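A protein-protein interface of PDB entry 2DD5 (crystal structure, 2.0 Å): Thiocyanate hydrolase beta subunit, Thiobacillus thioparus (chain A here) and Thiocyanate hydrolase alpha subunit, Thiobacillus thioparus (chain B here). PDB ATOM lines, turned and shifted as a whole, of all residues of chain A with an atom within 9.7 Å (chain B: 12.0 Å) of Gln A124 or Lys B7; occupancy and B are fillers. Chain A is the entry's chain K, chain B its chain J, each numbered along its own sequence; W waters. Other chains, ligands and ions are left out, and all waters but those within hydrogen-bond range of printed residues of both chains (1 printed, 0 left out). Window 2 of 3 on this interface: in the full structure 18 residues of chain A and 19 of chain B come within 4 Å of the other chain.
The backbone carbonyl oxygen (O) of Lys A123 is in hydrogen-bond range of the indole nitrogen (NE1) of Trp B10.
The backbone carbonyl oxygen (O) of Val A84 is in hydrogen-bond range of the side-chain amino group (NZ) of Lys A123 (2.7 Å). N of Phe A125 sits at hydrogen-bond distance from O of Leu A120 (2.8 Å).
Among the printed residues, merely in contact across the chains: Gln A124 with Pro B8 (3.2 Å), Phe A125 with Arg B12 (3.4 Å), Gln A124 with Lys B7 (3.9 Å) and Val A84 with Arg B12 (3.99 Å).
Gln A124 touches two residues of chain B. Of chain A, only Gln A124 comes within 4 Å of Lys B7. No residue of chain B comes within 4 Å of Val A121. No residue of chain B comes within 4 Å of Asp A122. Phe A125 touches just one residue of chain B: Arg B12. Thr A127 touches none of the printed residues of chain B. Of the printed residues of chain B, Val A84 touches Arg B12 (3.99 Å). Printed residues of chain A within 4 Å of Arg B12: Val A84 (3.99 Å) and Phe A125 (3.4 Å). The nearest residue of chain B that does not touch Gln A124 is Trp B10 (5.1 Å). The nearest residue of chain A that does not touch Lys B7 is Thr A127 (4.9 Å). The nearest printed residue of chain A that does not touch Trp B10 is Phe A125 (4.3 Å).
Of the 16 printed residues of chain A, 4 touch a printed residue of chain B. Hydrophobic or aromatic side chains of chain A that line the printed part of chain B: Val A84 and Phe A125. Of the 6 printed residues of chain B, 4 touch a printed residue of chain A. Hydrophobic or aromatic side chains of chain B that line the printed part of chain A: Pro B8 and Trp B10. Among the printed residues, 5 pairs touch across the chains.
Water W1 bridges O of Pro B8 (2.7 Å) and OE1 of Gln A124 (3.2 Å).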
ATOM      1  N   VAL A  84      30.507 -20.711   9.602  1.00  0.00           N
ATOM      2  CA  VAL A  84      29.122 -20.303   9.816  1.00  0.00           C
ATOM      3  C   VAL A  84      28.276 -20.924   8.699  1.00  0.00           C
ATOM      4  O   VAL A  84      27.092 -21.218   8.879  1.00  0.00           O
ATOM      5  CB  VAL A  84      28.982 -18.764   9.804  1.00  0.00           C
ATOM      6  CG1 VAL A  84      27.510 -18.372   9.733  1.00  0.00           C
ATOM      7  CG2 VAL A  84      29.612 -18.180  11.072  1.00  0.00           C
ATOM      8  N   LYS A  93      20.911 -19.761  -0.577  1.00  0.00           N
ATOM      9  CA  LYS A  93      20.187 -18.666   0.069  1.00  0.00           C
ATOM     10  C   LYS A  93      20.247 -17.375  -0.742  1.00  0.00           C
ATOM     11  O   LYS A  93      19.263 -16.651  -0.865  1.00  0.00           O
ATOM     12  CB  LYS A  93      20.778 -18.387   1.457  1.00  0.00           C
ATOM     13  CG  LYS A  93      20.736 -19.564   2.427  1.00  0.00           C
ATOM     14  CD  LYS A  93      21.504 -19.248   3.711  1.00  0.00           C
ATOM     15  CE  LYS A  93      20.803 -18.182   4.543  1.00  0.00           C
ATOM     16  NZ  LYS A  93      19.482 -18.654   5.032  1.00  0.00           N
ATOM     17  N   ALA A 116      24.300 -12.402   3.767  1.00  0.00           N
ATOM     18  CA  ALA A 116      25.269 -12.515   4.853  1.00  0.00           C
ATOM     19  C   ALA A 116      24.513 -12.159   6.138  1.00  0.00           C
ATOM     20  O   ALA A 116      24.691 -12.797   7.177  1.00  0.00           O
ATOM     21  CB  ALA A 116      26.426 -11.545   4.636  1.00  0.00           C
ATOM     22  N   ALA A 117      23.669 -11.135   6.058  1.00  0.00           N
ATOM     23  CA  ALA A 117      22.874 -10.721   7.211  1.00  0.00           C
ATOM     24  C   ALA A 117      21.885 -11.834   7.533  1.00  0.00           C
ATOM     25  O   ALA A 117      21.616 -12.137   8.695  1.00  0.00           O
ATOM     26  CB  ALA A 117      22.119  -9.436   6.893  1.00  0.00           C
ATOM     27  N   ARG A 118      21.352 -12.446   6.483  1.00  0.00           N
ATOM     28  CA  ARG A 118      20.377 -13.510   6.629  1.00  0.00           C
ATOM     29  C   ARG A 118      20.920 -14.722   7.386  1.00  0.00           C
ATOM     30  O   ARG A 118      20.257 -15.248   8.281  1.00  0.00           O
ATOM     31  CB  ARG A 118      19.876 -13.940   5.241  1.00  0.00           C
ATOM     32  CG  ARG A 118      18.742 -14.925   5.280  1.00  0.00           C
ATOM     33  CD  ARG A 118      17.417 -14.260   5.651  1.00  0.00           C
ATOM     34  NE  ARG A 118      16.479 -15.257   6.151  1.00  0.00           N
ATOM     35  CZ  ARG A 118      15.156 -15.154   6.086  1.00  0.00           C
ATOM     36  NH1 ARG A 118      14.589 -14.089   5.530  1.00  0.00           N
ATOM     37  NH2 ARG A 118      14.404 -16.120   6.590  1.00  0.00           N
ATOM     38  N   ILE A 119      22.123 -15.168   7.042  1.00  0.00           N
ATOM     39  CA  ILE A 119      22.677 -16.335   7.714  1.00  0.00           C
ATOM     40  C   ILE A 119      22.874 -16.090   9.216  1.00  0.00           C
ATOM     41  O   ILE A 119      22.662 -16.992  10.027  1.00  0.00           O
ATOM     42  CB  ILE A 119      24.011 -16.788   7.056  1.00  0.00           C
ATOM     43  CG1 ILE A 119      24.415 -18.165   7.591  1.00  0.00           C
ATOM     44  CG2 ILE A 119      25.111 -15.769   7.315  1.00  0.00           C
ATOM     45  CD1 ILE A 119      23.457 -19.290   7.209  1.00  0.00           C
ATOM     46  N   LEU A 120      23.261 -14.874   9.592  1.00  0.00           N
ATOM     47  CA  LEU A 120      23.459 -14.563  11.013  1.00  0.00           C
ATOM     48  C   LEU A 120      22.160 -14.779  11.787  1.00  0.00           C
ATOM     49  O   LEU A 120      22.166 -15.291  12.908  1.00  0.00           O
ATOM     50  CB  LEU A 120      23.908 -13.112  11.197  1.00  0.00           C
ATOM     51  CG  LEU A 120      25.208 -12.674  10.520  1.00  0.00           C
ATOM     52  CD1 LEU A 120      25.567 -11.264  10.968  1.00  0.00           C
ATOM     53  CD2 LEU A 120      26.316 -13.637  10.870  1.00  0.00           C
ATOM     54  N   VAL A 121      21.045 -14.388  11.179  1.00  0.00           N
ATOM     55  CA  VAL A 121      19.740 -14.539  11.815  1.00  0.00           C
ATOM     56  C   VAL A 121      19.190 -15.962  11.709  1.00  0.00           C
ATOM     57  O   VAL A 121      18.708 -16.523  12.699  1.00  0.00           O
ATOM     58  CB  VAL A 121      18.714 -13.561  11.206  1.00  0.00           C
ATOM     59  CG1 VAL A 121      17.349 -13.763  11.853  1.00  0.00           C
ATOM     60  CG2 VAL A 121      19.189 -12.130  11.410  1.00  0.00           C
ATOM     61  N   ASP A 122      19.266 -16.553  10.519  1.00  0.00           N
ATOM     62  CA  ASP A 122      18.746 -17.903  10.340  1.00  0.00           C
ATOM     63  C   ASP A 122      19.418 -18.940  11.236  1.00  0.00           C
ATOM     64  O   ASP A 122      18.751 -19.843  11.741  1.00  0.00           O
ATOM     65  CB  ASP A 122      18.835 -18.332   8.870  1.00  0.00           C
ATOM     66  CG  ASP A 122      17.764 -17.674   8.007  1.00  0.00           C
ATOM     67  OD1 ASP A 122      16.630 -17.499   8.501  1.00  0.00           O
ATOM     68  OD2 ASP A 122      18.042 -17.344   6.835  1.00  0.00           O
ATOM     69  N   LYS A 123      20.726 -18.820  11.445  1.00  0.00           N
ATOM     70  CA  LYS A 123      21.408 -19.774  12.316  1.00  0.00           C
ATOM     71  C   LYS A 123      21.476 -19.277  13.761  1.00  0.00           C
ATOM     72  O   LYS A 123      22.199 -19.822  14.596  1.00  0.00           O
ATOM     73  CB  LYS A 123      22.798 -20.106  11.771  1.00  0.00           C
ATOM     74  CG  LYS A 123      22.720 -21.017  10.545  1.00  0.00           C
ATOM     75  CD  LYS A 123      24.066 -21.579  10.128  1.00  0.00           C
ATOM     76  CE  LYS A 123      23.888 -22.567   8.975  1.00  0.00           C
ATOM     77  NZ  LYS A 123      25.182 -23.056   8.420  1.00  0.00           N
ATOM     78  N   GLN A 124      20.707 -18.231  14.034  1.00  0.00           N
ATOM     79  CA  GLN A 124      20.595 -17.659  15.369  1.00  0.00           C
ATOM     80  C   GLN A 124      21.873 -17.159  16.043  1.00  0.00           C
ATOM     81  O   GLN A 124      21.988 -17.212  17.269  1.00  0.00           O
ATOM     82  CB  GLN A 124      19.886 -18.671  16.278  1.00  0.00           C
ATOM     83  CG  GLN A 124      18.508 -19.081  15.757  1.00  0.00           C
ATOM     84  CD  GLN A 124      17.851 -20.176  16.586  1.00  0.00           C
ATOM     85  OE1 GLN A 124      18.395 -21.266  16.738  1.00  0.00           O
ATOM     86  NE2 GLN A 124      16.674 -19.887  17.120  1.00  0.00           N
ATOM     87  N   PHE A 125      22.831 -16.673  15.259  1.00  0.00           N
ATOM     88  CA  PHE A 125      24.054 -16.142  15.845  1.00  0.00           C
ATOM     89  C   PHE A 125      23.744 -14.744  16.367  1.00  0.00           C
ATOM     90  O   PHE A 125      24.401 -14.245  17.278  1.00  0.00           O
ATOM     91  CB  PHE A 125      25.188 -16.128  14.819  1.00  0.00           C
ATOM     92  CG  PHE A 125      25.732 -17.499  14.518  1.00  0.00           C
ATOM     93  CD1 PHE A 125      26.348 -18.247  15.516  1.00  0.00           C
ATOM     94  CD2 PHE A 125      25.594 -18.057  13.251  1.00  0.00           C
ATOM     95  CE1 PHE A 125      26.817 -19.535  15.259  1.00  0.00           C
ATOM     96  CE2 PHE A 125      26.060 -19.344  12.981  1.00  0.00           C
ATOM     97  CZ  PHE A 125      26.670 -20.084  13.986  1.00  0.00           C
ATOM     98  N   VAL A 126      22.730 -14.123  15.777  1.00  0.00           N
ATOM     99  CA  VAL A 126      22.250 -12.811  16.205  1.00  0.00           C
ATOM    100  C   VAL A 126      20.738 -12.902  16.078  1.00  0.00           C
ATOM    101  O   VAL A 126      20.230 -13.623  15.219  1.00  0.00           O
ATOM    102  CB  VAL A 126      22.736 -11.654  15.294  1.00  0.00           C
ATOM    103  CG1 VAL A 126      24.247 -11.699  15.140  1.00  0.00           C
ATOM    104  CG2 VAL A 126      22.047 -11.727  13.940  1.00  0.00           C
ATOM    105  N   THR A 127      20.011 -12.200  16.936  1.00  0.00           N
ATOM    106  CA  THR A 127      18.560 -12.217  16.836  1.00  0.00           C
ATOM    107  C   THR A 127      18.199 -11.154  15.801  1.00  0.00           C
ATOM    108  O   THR A 127      19.004 -10.261  15.516  1.00  0.00           O
ATOM    109  CB  THR A 127      17.893 -11.842  18.174  1.00  0.00           C
ATOM    110  OG1 THR A 127      18.315 -10.528  18.558  1.00  0.00           O
ATOM    111  CG2 THR A 127      18.274 -12.847  19.270  1.00  0.00           C
ATOM    112  N   LEU A 128      17.007 -11.242  15.224  1.00  0.00           N
ATOM    113  CA  LEU A 128      16.613 -10.236  14.251  1.00  0.00           C
ATOM    114  C   LEU A 128      16.566  -8.892  14.976  1.00  0.00           C
ATOM    115  O   LEU A 128      16.828  -7.843  14.390  1.00  0.00           O
ATOM    116  CB  LEU A 128      15.243 -10.557  13.650  1.00  0.00           C
ATOM    117  CG  LEU A 128      14.801  -9.593  12.545  1.00  0.00           C
ATOM    118  CD1 LEU A 128      15.858  -9.557  11.444  1.00  0.00           C
ATOM    119  CD2 LEU A 128      13.455 -10.026  11.987  1.00  0.00           C
ATOM    120  N   GLU A 130      18.582  -7.855  17.336  1.00  0.00           N
ATOM    121  CA  GLU A 130      19.946  -7.343  17.384  1.00  0.00           C
ATOM    122  C   GLU A 130      20.345  -6.736  16.041  1.00  0.00           C
ATOM    123  O   GLU A 130      21.024  -5.713  15.995  1.00  0.00           O
ATOM    124  CB  GLU A 130      20.927  -8.462  17.756  1.00  0.00           C
ATOM    125  CG  GLU A 130      20.822  -8.928  19.209  1.00  0.00           C
ATOM    126  CD  GLU A 130      21.800 -10.044  19.544  1.00  0.00           C
ATOM    127  OE1 GLU A 130      21.772 -11.088  18.856  1.00  0.00           O
ATOM    128  OE2 GLU A 130      22.594  -9.881  20.496  1.00  0.00           O
ATOM    129  N   LYS B   7      17.970 -24.222  22.008  1.00  0.00           N
ATOM    130  CA  LYS B   7      18.329 -23.777  20.628  1.00  0.00           C
ATOM    131  C   LYS B   7      19.418 -24.643  20.006  1.00  0.00           C
ATOM    132  O   LYS B   7      20.291 -25.163  20.701  1.00  0.00           O
ATOM    133  CB  LYS B   7      18.789 -22.319  20.639  1.00  0.00           C
ATOM    134  CG  LYS B   7      17.669 -21.318  20.858  1.00  0.00           C
ATOM    135  CD  LYS B   7      18.192 -19.897  20.726  1.00  0.00           C
ATOM    136  CE  LYS B   7      17.078 -18.879  20.868  1.00  0.00           C
ATOM    137  NZ  LYS B   7      17.611 -17.486  20.827  1.00  0.00           N
ATOM    138  N   PRO B   8      19.380 -24.800  18.673  1.00  0.00           N
ATOM    139  CA  PRO B   8      20.349 -25.603  17.923  1.00  0.00           C
ATOM    140  C   PRO B   8      21.781 -25.094  18.021  1.00  0.00           C
ATOM    141  O   PRO B   8      22.021 -23.895  18.146  1.00  0.00           O
ATOM    142  CB  PRO B   8      19.825 -25.529  16.490  1.00  0.00           C
ATOM    143  CG  PRO B   8      18.362 -25.309  16.670  1.00  0.00           C
ATOM    144  CD  PRO B   8      18.327 -24.296  17.777  1.00  0.00           C
ATOM    145  N   VAL B   9      22.728 -26.021  17.964  1.00  0.00           N
ATOM    146  CA  VAL B   9      24.138 -25.673  18.006  1.00  0.00           C
ATOM    147  C   VAL B   9      24.730 -26.075  16.661  1.00  0.00           C
ATOM    148  O   VAL B   9      24.494 -27.186  16.183  1.00  0.00           O
ATOM    149  CB  VAL B   9      24.884 -26.431  19.124  1.00  0.00           C
ATOM    150  CG1 VAL B   9      26.358 -26.067  19.097  1.00  0.00           C
ATOM    151  CG2 VAL B   9      24.285 -26.090  20.478  1.00  0.00           C
ATOM    152  N   TRP B  10      25.483 -25.169  16.046  1.00  0.00           N
ATOM    153  CA  TRP B  10      26.097 -25.454  14.755  1.00  0.00           C
ATOM    154  C   TRP B  10      27.592 -25.673  14.908  1.00  0.00           C
ATOM    155  O   TRP B  10      28.309 -24.807  15.411  1.00  0.00           O
ATOM    156  CB  TRP B  10      25.846 -24.307  13.776  1.00  0.00           C
ATOM    157  CG  TRP B  10      24.408 -23.941  13.669  1.00  0.00           C
ATOM    158  CD1 TRP B  10      23.711 -23.110  14.498  1.00  0.00           C
ATOM    159  CD2 TRP B  10      23.468 -24.438  12.714  1.00  0.00           C
ATOM    160  NE1 TRP B  10      22.392 -23.060  14.118  1.00  0.00           N
ATOM    161  CE2 TRP B  10      22.215 -23.866  13.026  1.00  0.00           C
ATOM    162  CE3 TRP B  10      23.561 -25.313  11.623  1.00  0.00           C
ATOM    163  CZ2 TRP B  10      21.062 -24.141  12.287  1.00  0.00           C
ATOM    164  CZ3 TRP B  10      22.414 -25.586  10.888  1.00  0.00           C
ATOM    165  CH2 TRP B  10      21.180 -25.001  11.224  1.00  0.00           C
ATOM    166  N   ASP B  11      28.053 -26.841  14.476  1.00  0.00           N
ATOM    167  CA  ASP B  11      29.464 -27.190  14.549  1.00  0.00           C
ATOM    168  C   ASP B  11      30.212 -26.352  13.518  1.00  0.00           C
ATOM    169  O   ASP B  11      30.180 -26.655  12.325  1.00  0.00           O
ATOM    170  CB  ASP B  11      29.641 -28.673  14.237  1.00  0.00           C
ATOM    171  CG  ASP B  11      31.084 -29.115  14.315  1.00  0.00           C
ATOM    172  OD1 ASP B  11      31.962 -28.368  13.832  1.00  0.00           O
ATOM    173  OD2 ASP B  11      31.337 -30.213  14.847  1.00  0.00           O
ATOM    174  N   ARG B  12      30.897 -25.310  13.972  1.00  0.00           N
ATOM    175  CA  ARG B  12      31.616 -24.441  13.051  1.00  0.00           C
ATOM    176  C   ARG B  12      33.059 -24.847  12.771  1.00  0.00           C
ATOM    177  O   ARG B  12      33.765 -24.158  12.039  1.00  0.00           O
ATOM    178  CB  ARG B  12      31.578 -22.999  13.566  1.00  0.00           C
ATOM    179  CG  ARG B  12      30.203 -22.575  14.048  1.00  0.00           C
ATOM    180  CD  ARG B  12      29.917 -21.119  13.759  1.00  0.00           C
ATOM    181  NE  ARG B  12      30.837 -20.198  14.417  1.00  0.00           N
ATOM    182  CZ  ARG B  12      30.934 -20.029  15.732  1.00  0.00           C
ATOM    183  NH1 ARG B  12      30.166 -20.726  16.557  1.00  0.00           N
ATOM    184  NH2 ARG B  12      31.790 -19.142  16.220  1.00  0.00           N
HETATM  185  O   HOH W   1      21.272 -21.293  18.175  1.00  0.00           O
